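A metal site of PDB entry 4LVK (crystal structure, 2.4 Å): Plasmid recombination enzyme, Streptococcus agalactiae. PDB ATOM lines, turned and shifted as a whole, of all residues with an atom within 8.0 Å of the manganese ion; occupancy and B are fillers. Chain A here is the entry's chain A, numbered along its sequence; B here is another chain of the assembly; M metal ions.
Of the 22 residues printed, 6 come within 4 Å of the manganese ion. The nearest printed residue that does not touch the manganese ion is Arg 24 (4.1 Å).
OE2 of Glu 128 binds the manganese ion (1.9 Å). NE2 of His 132 binds the manganese ion, 2.0 Å away. A ring nitrogen (ND1) of His 125 binds the manganese ion (2.0 Å). NE2 of His 134 binds the manganese ion, at 2.1 Å. The manganese ion is bound by OP1 of DT 16 of chain B, 2.2 Å away. The manganese ion is bound by O3' of DG 15 of chain B, 2.6 Å away.
The side-chain carboxylate of Glu 81 lies within hydrogen-bond range of a ring nitrogen (ND1) of His 134 (3.1 Å). OP1 of DG 15 of chain B is in hydrogen-bond range of the side-chain hydroxyl (OG) of Ser 129 (2.7 Å). The backbone carbonyl oxygen of Thr 130 is in hydrogen-bond range of a ring nitrogen (ND1) of His 132. The side-chain amide nitrogen (ND2) of Asn 31 sits at hydrogen-bond distance from OP2 of DG 15 of chain B (3.5 Å). ND1 of His 125 sits close to NH2 of Arg 24 (3.3 Å). The backbone carbonyl oxygen (O) of Ser 123 is in hydrogen-bond range of the backbone NH (N) of His 134, 2.8 Å away. A ring nitrogen (NE2) of His 125 sits at hydrogen-bond distance from the backbone carbonyl oxygen of Asn 22 (3.3 Å). OE1 of Glu 128 lies within salt-bridge range of NH2 of Arg 24, at 3.9 Å.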
ATOM      1  N   HIS A  21      -5.559  -0.585  -5.464  1.00  0.00           N
ATOM      2  CA  HIS A  21      -6.987  -0.277  -5.391  1.00  0.00           C
ATOM      3  C   HIS A  21      -7.775  -1.399  -4.774  1.00  0.00           C
ATOM      4  O   HIS A  21      -8.562  -1.133  -3.887  1.00  0.00           O
ATOM      5  CB  HIS A  21      -7.593   0.108  -6.739  1.00  0.00           C
ATOM      6  CG  HIS A  21      -6.878   1.217  -7.434  1.00  0.00           C
ATOM      7  ND1 HIS A  21      -6.823   1.318  -8.812  1.00  0.00           N
ATOM      8  CD2 HIS A  21      -6.157   2.259  -6.954  1.00  0.00           C
ATOM      9  CE1 HIS A  21      -6.105   2.372  -9.148  1.00  0.00           C
ATOM     10  NE2 HIS A  21      -5.685   2.954  -8.038  1.00  0.00           N
ATOM     11  N   ASN A  22      -7.577  -2.643  -5.234  1.00  0.00           N
ATOM     12  CA  ASN A  22      -8.448  -3.758  -4.802  1.00  0.00           C
ATOM     13  C   ASN A  22      -8.364  -3.966  -3.291  1.00  0.00           C
ATOM     14  O   ASN A  22      -9.310  -4.505  -2.719  1.00  0.00           O
ATOM     15  CB  ASN A  22      -8.198  -5.133  -5.495  1.00  0.00           C
ATOM     16  CG  ASN A  22      -8.624  -5.191  -6.980  1.00  0.00           C
ATOM     17  OD1 ASN A  22      -9.024  -4.197  -7.640  1.00  0.00           O
ATOM     18  ND2 ASN A  22      -8.493  -6.399  -7.540  1.00  0.00           N
ATOM     19  N   ARG A  24      -7.787  -1.328  -1.158  1.00  0.00           N
ATOM     20  CA  ARG A  24      -8.079   0.000  -0.582  1.00  0.00           C
ATOM     21  C   ARG A  24      -6.902   0.458   0.248  1.00  0.00           C
ATOM     22  O   ARG A  24      -7.051   0.828   1.421  1.00  0.00           O
ATOM     23  CB  ARG A  24      -9.391   0.021   0.219  1.00  0.00           C
ATOM     24  CG  ARG A  24     -10.611  -0.405  -0.603  1.00  0.00           C
ATOM     25  CD  ARG A  24     -11.049   0.695  -1.554  1.00  0.00           C
ATOM     26  NE  ARG A  24     -12.278   0.379  -2.274  1.00  0.00           N
ATOM     27  CZ  ARG A  24     -12.340  -0.110  -3.512  1.00  0.00           C
ATOM     28  NH1 ARG A  24     -11.219  -0.380  -4.201  1.00  0.00           N
ATOM     29  NH2 ARG A  24     -13.552  -0.344  -4.057  1.00  0.00           N
ATOM     30  N   ASN A  31     -11.836   7.822  -5.564  1.00  0.00           N
ATOM     31  CA  ASN A  31     -12.920   7.838  -6.561  1.00  0.00           C
ATOM     32  C   ASN A  31     -14.180   8.364  -5.853  1.00  0.00           C
ATOM     33  O   ASN A  31     -14.434   8.049  -4.676  1.00  0.00           O
ATOM     34  CB  ASN A  31     -13.077   6.442  -7.235  1.00  0.00           C
ATOM     35  CG  ASN A  31     -14.484   6.154  -7.781  1.00  0.00           C
ATOM     36  OD1 ASN A  31     -15.339   7.029  -7.876  1.00  0.00           O
ATOM     37  ND2 ASN A  31     -14.730   4.887  -8.140  1.00  0.00           N
ATOM     38  N   ILE A  34     -16.675   5.734  -4.297  1.00  0.00           N
ATOM     39  CA  ILE A  34     -16.271   4.840  -3.207  1.00  0.00           C
ATOM     40  C   ILE A  34     -16.759   5.453  -1.885  1.00  0.00           C
ATOM     41  O   ILE A  34     -16.453   6.600  -1.592  1.00  0.00           O
ATOM     42  CB  ILE A  34     -14.750   4.582  -3.211  1.00  0.00           C
ATOM     43  CG1 ILE A  34     -14.378   3.773  -4.444  1.00  0.00           C
ATOM     44  CG2 ILE A  34     -14.315   3.858  -1.950  1.00  0.00           C
ATOM     45  CD1 ILE A  34     -12.902   3.823  -4.792  1.00  0.00           C
ATOM     46  N   ASN A  42     -15.826  -4.763   2.388  1.00  0.00           N
ATOM     47  CA  ASN A  42     -15.328  -5.599   1.313  1.00  0.00           C
ATOM     48  C   ASN A  42     -14.757  -6.907   1.877  1.00  0.00           C
ATOM     49  O   ASN A  42     -14.505  -6.996   3.087  1.00  0.00           O
ATOM     50  CB  ASN A  42     -14.278  -4.842   0.515  1.00  0.00           C
ATOM     51  CG  ASN A  42     -14.838  -3.604  -0.185  1.00  0.00           C
ATOM     52  OD1 ASN A  42     -16.073  -3.378  -0.246  1.00  0.00           O
ATOM     53  ND2 ASN A  42     -13.905  -2.765  -0.724  1.00  0.00           N
ATOM     54  N   GLU A  81      -8.245 -10.422 -15.556  1.00  0.00           N
ATOM     55  CA  GLU A  81      -9.114  -9.973 -14.457  1.00  0.00           C
ATOM     56  C   GLU A  81     -10.546  -9.946 -14.959  1.00  0.00           C
ATOM     57  O   GLU A  81     -10.864  -9.205 -15.857  1.00  0.00           O
ATOM     58  CB  GLU A  81      -8.712  -8.611 -13.833  1.00  0.00           C
ATOM     59  CG  GLU A  81      -9.565  -8.296 -12.610  1.00  0.00           C
ATOM     60  CD  GLU A  81      -9.317  -6.952 -11.955  1.00  0.00           C
ATOM     61  OE1 GLU A  81     -10.124  -6.036 -12.186  1.00  0.00           O
ATOM     62  OE2 GLU A  81      -8.364  -6.790 -11.152  1.00  0.00           O
ATOM     63  N   ILE A  83     -14.401  -9.062 -14.243  1.00  0.00           N
ATOM     64  CA  ILE A  83     -15.382  -8.354 -13.424  1.00  0.00           C
ATOM     65  C   ILE A  83     -16.702  -9.172 -13.476  1.00  0.00           C
ATOM     66  O   ILE A  83     -17.261  -9.433 -14.564  1.00  0.00           O
ATOM     67  CB  ILE A  83     -15.627  -6.886 -13.874  1.00  0.00           C
ATOM     68  CG1 ILE A  83     -14.361  -6.055 -13.783  1.00  0.00           C
ATOM     69  CG2 ILE A  83     -16.658  -6.204 -12.967  1.00  0.00           C
ATOM     70  CD1 ILE A  83     -13.648  -6.139 -12.445  1.00  0.00           C
ATOM     71  N   SER A 123     -11.925 -10.568  -5.292  1.00  0.00           N
ATOM     72  CA  SER A 123     -12.003  -9.442  -4.378  1.00  0.00           C
ATOM     73  C   SER A 123     -13.350  -8.788  -4.591  1.00  0.00           C
ATOM     74  O   SER A 123     -13.616  -8.250  -5.683  1.00  0.00           O
ATOM     75  CB  SER A 123     -10.839  -8.515  -4.692  1.00  0.00           C
ATOM     76  OG  SER A 123     -10.848  -7.426  -3.819  1.00  0.00           O
ATOM     77  N   VAL A 124     -14.203  -8.870  -3.565  1.00  0.00           N
ATOM     78  CA  VAL A 124     -15.604  -8.419  -3.619  1.00  0.00           C
ATOM     79  C   VAL A 124     -15.749  -7.006  -3.051  1.00  0.00           C
ATOM     80  O   VAL A 124     -15.440  -6.738  -1.861  1.00  0.00           O
ATOM     81  CB  VAL A 124     -16.552  -9.392  -2.859  1.00  0.00           C
ATOM     82  CG1 VAL A 124     -18.015  -8.940  -2.940  1.00  0.00           C
ATOM     83  CG2 VAL A 124     -16.369 -10.826  -3.366  1.00  0.00           C
ATOM     84  N   HIS A 125     -16.237  -6.108  -3.896  1.00  0.00           N
ATOM     85  CA  HIS A 125     -16.346  -4.723  -3.537  1.00  0.00           C
ATOM     86  C   HIS A 125     -17.808  -4.378  -3.244  1.00  0.00           C
ATOM     87  O   HIS A 125     -18.673  -4.431  -4.158  1.00  0.00           O
ATOM     88  CB  HIS A 125     -15.804  -3.868  -4.654  1.00  0.00           C
ATOM     89  CG  HIS A 125     -14.314  -3.835  -4.735  1.00  0.00           C
ATOM     90  ND1 HIS A 125     -13.649  -3.186  -5.765  1.00  0.00           N
ATOM     91  CD2 HIS A 125     -13.368  -4.339  -3.904  1.00  0.00           C
ATOM     92  CE1 HIS A 125     -12.339  -3.297  -5.540  1.00  0.00           C
ATOM     93  NE2 HIS A 125     -12.140  -3.991  -4.428  1.00  0.00           N
ATOM     94  N   LEU A 126     -18.084  -4.044  -1.986  1.00  0.00           N
ATOM     95  CA  LEU A 126     -19.412  -3.597  -1.551  1.00  0.00           C
ATOM     96  C   LEU A 126     -19.425  -2.129  -1.218  1.00  0.00           C
ATOM     97  O   LEU A 126     -20.398  -1.655  -0.654  1.00  0.00           O
ATOM     98  CB  LEU A 126     -19.904  -4.381  -0.338  1.00  0.00           C
ATOM     99  CG  LEU A 126     -19.956  -5.892  -0.583  1.00  0.00           C
ATOM    100  CD1 LEU A 126     -20.372  -6.619   0.697  1.00  0.00           C
ATOM    101  CD2 LEU A 126     -20.908  -6.217  -1.698  1.00  0.00           C
ATOM    102  N   ASP A 127     -18.355  -1.406  -1.568  1.00  0.00           N
ATOM    103  CA  ASP A 127     -18.253  -0.022  -1.168  1.00  0.00           C
ATOM    104  C   ASP A 127     -18.387   0.925  -2.340  1.00  0.00           C
ATOM    105  O   ASP A 127     -18.139   2.118  -2.187  1.00  0.00           O
ATOM    106  CB  ASP A 127     -16.955   0.232  -0.385  1.00  0.00           C
ATOM    107  CG  ASP A 127     -15.649  -0.060  -1.208  1.00  0.00           C
ATOM    108  OD1 ASP A 127     -15.638  -0.684  -2.312  1.00  0.00           O
ATOM    109  OD2 ASP A 127     -14.578   0.319  -0.674  1.00  0.00           O
ATOM    110  N   GLU A 128     -18.770   0.387  -3.491  1.00  0.00           N
ATOM    111  CA  GLU A 128     -18.948   1.200  -4.708  1.00  0.00           C
ATOM    112  C   GLU A 128     -20.446   1.299  -5.017  1.00  0.00           C
ATOM    113  O   GLU A 128     -21.252   1.091  -4.113  1.00  0.00           O
ATOM    114  CB  GLU A 128     -18.081   0.663  -5.875  1.00  0.00           C
ATOM    115  CG  GLU A 128     -16.683   0.241  -5.434  1.00  0.00           C
ATOM    116  CD  GLU A 128     -15.658   0.312  -6.504  1.00  0.00           C
ATOM    117  OE1 GLU A 128     -15.427   1.452  -6.957  1.00  0.00           O
ATOM    118  OE2 GLU A 128     -15.065  -0.750  -6.845  1.00  0.00           O
ATOM    119  N   SER A 129     -20.842   1.629  -6.243  1.00  0.00           N
ATOM    120  CA  SER A 129     -22.272   1.679  -6.575  1.00  0.00           C
ATOM    121  C   SER A 129     -23.034   0.352  -6.491  1.00  0.00           C
ATOM    122  O   SER A 129     -24.185   0.367  -6.056  1.00  0.00           O
ATOM    123  CB  SER A 129     -22.531   2.330  -7.933  1.00  0.00           C
ATOM    124  OG  SER A 129     -22.021   3.643  -7.905  1.00  0.00           O
ATOM    125  N   THR A 130     -22.435  -0.781  -6.881  1.00  0.00           N
ATOM    126  CA  THR A 130     -23.184  -2.067  -7.008  1.00  0.00           C
ATOM    127  C   THR A 130     -22.226  -3.152  -6.614  1.00  0.00           C
ATOM    128  O   THR A 130     -21.088  -3.113  -7.022  1.00  0.00           O
ATOM    129  CB  THR A 130     -23.534  -2.371  -8.476  1.00  0.00           C
ATOM    130  OG1 THR A 130     -24.239  -1.279  -9.043  1.00  0.00           O
ATOM    131  CG2 THR A 130     -24.375  -3.653  -8.650  1.00  0.00           C
ATOM    132  N   PRO A 131     -22.692  -4.159  -5.873  1.00  0.00           N
ATOM    133  CA  PRO A 131     -21.739  -5.216  -5.577  1.00  0.00           C
ATOM    134  C   PRO A 131     -21.110  -5.829  -6.863  1.00  0.00           C
ATOM    135  O   PRO A 131     -21.809  -6.102  -7.863  1.00  0.00           O
ATOM    136  CB  PRO A 131     -22.553  -6.225  -4.777  1.00  0.00           C
ATOM    137  CG  PRO A 131     -23.641  -5.392  -4.146  1.00  0.00           C
ATOM    138  CD  PRO A 131     -23.933  -4.255  -5.067  1.00  0.00           C
ATOM    139  N   HIS A 132     -19.781  -5.976  -6.853  1.00  0.00           N
ATOM    140  CA  HIS A 132     -19.079  -6.617  -7.961  1.00  0.00           C
ATOM    141  C   HIS A 132     -17.846  -7.287  -7.380  1.00  0.00           C
ATOM    142  O   HIS A 132     -17.437  -6.970  -6.247  1.00  0.00           O
ATOM    143  CB  HIS A 132     -18.731  -5.589  -9.048  1.00  0.00           C
ATOM    144  CG  HIS A 132     -17.789  -4.510  -8.581  1.00  0.00           C
ATOM    145  ND1 HIS A 132     -18.235  -3.374  -7.916  1.00  0.00           N
ATOM    146  CD2 HIS A 132     -16.445  -4.396  -8.669  1.00  0.00           C
ATOM    147  CE1 HIS A 132     -17.200  -2.607  -7.634  1.00  0.00           C
ATOM    148  NE2 HIS A 132     -16.097  -3.207  -8.073  1.00  0.00           N
ATOM    149  N   MET A 133     -17.257  -8.192  -8.164  1.00  0.00           N
ATOM    150  CA  MET A 133     -16.037  -8.875  -7.805  1.00  0.00           C
ATOM    151  C   MET A 133     -14.967  -8.718  -8.896  1.00  0.00           C
ATOM    152  O   MET A 133     -15.307  -8.839 -10.082  1.00  0.00           O
ATOM    153  CB  MET A 133     -16.335 -10.352  -7.545  1.00  0.00           C
ATOM    154  CG  MET A 133     -15.117 -11.262  -7.531  1.00  0.00           C
ATOM    155  SD  MET A 133     -15.534 -12.876  -6.876  1.00  0.00           S
ATOM    156  CE  MET A 133     -16.261 -13.671  -8.320  1.00  0.00           C
ATOM    157  N   HIS A 134     -13.726  -8.438  -8.474  1.00  0.00           N
ATOM    158  CA  HIS A 134     -12.546  -8.336  -9.387  1.00  0.00           C
ATOM    159  C   HIS A 134     -11.817  -9.673  -9.113  1.00  0.00           C
ATOM    160  O   HIS A 134     -11.327  -9.901  -7.976  1.00  0.00           O
ATOM    161  CB  HIS A 134     -11.586  -7.148  -9.074  1.00  0.00           C
ATOM    162  CG  HIS A 134     -12.228  -5.780  -9.025  1.00  0.00           C
ATOM    163  ND1 HIS A 134     -11.992  -4.820  -9.987  1.00  0.00           N
ATOM    164  CD2 HIS A 134     -13.050  -5.195  -8.103  1.00  0.00           C
ATOM    165  CE1 HIS A 134     -12.666  -3.716  -9.680  1.00  0.00           C
ATOM    166  NE2 HIS A 134     -13.321  -3.907  -8.547  1.00  0.00           N
ATOM    167  P    DG B  15     -18.649   2.664  -9.769  1.00  0.00           P
ATOM    168  OP1  DG B  15     -19.653   2.651  -8.679  1.00  0.00           O
ATOM    169  OP2  DG B  15     -17.531   3.621  -9.711  1.00  0.00           O
ATOM    170  O5'  DG B  15     -18.030   1.219  -9.985  1.00  0.00           O
ATOM    171  C5'  DG B  15     -16.908   1.043 -10.857  1.00  0.00           C
ATOM    172  C4'  DG B  15     -16.481  -0.396 -10.819  1.00  0.00           C
ATOM    173  O4'  DG B  15     -17.114  -1.076 -11.915  1.00  0.00           O
ATOM    174  C3'  DG B  15     -14.995  -0.654 -11.001  1.00  0.00           C
ATOM    175  O3'  DG B  15     -14.448  -0.945  -9.728  1.00  0.00           O
ATOM    176  C2'  DG B  15     -14.930  -2.020 -11.683  1.00  0.00           C
ATOM    177  C1'  DG B  15     -16.347  -2.215 -12.236  1.00  0.00           C
ATOM    178  N9   DG B  15     -16.406  -2.414 -13.686  1.00  0.00           N
ATOM    179  C8   DG B  15     -15.359  -2.367 -14.573  1.00  0.00           C
ATOM    180  N7   DG B  15     -15.723  -2.568 -15.808  1.00  0.00           N
ATOM    181  C5   DG B  15     -17.099  -2.774 -15.729  1.00  0.00           C
ATOM    182  C6   DG B  15     -18.042  -3.058 -16.756  1.00  0.00           C
ATOM    183  O6   DG B  15     -17.856  -3.180 -17.967  1.00  0.00           O
ATOM    184  N1   DG B  15     -19.316  -3.227 -16.230  1.00  0.00           N
ATOM    185  C2   DG B  15     -19.655  -3.112 -14.902  1.00  0.00           C
ATOM    186  N2   DG B  15     -20.944  -3.287 -14.604  1.00  0.00           N
ATOM    187  N3   DG B  15     -18.777  -2.836 -13.949  1.00  0.00           N
ATOM    188  C4   DG B  15     -17.530  -2.691 -14.427  1.00  0.00           C
ATOM    189  P    DT B  16     -13.114  -0.244  -9.146  1.00  0.00           P
ATOM    190  OP1  DT B  16     -12.666  -1.075  -8.038  1.00  0.00           O
ATOM    191  OP2  DT B  16     -13.457   1.200  -8.809  1.00  0.00           O
ATOM    192  O5'  DT B  16     -12.083  -0.370 -10.350  1.00  0.00           O
HETATM  193 MN    MN M   1     -14.310  -2.406  -7.524  1.00  0.00          MN
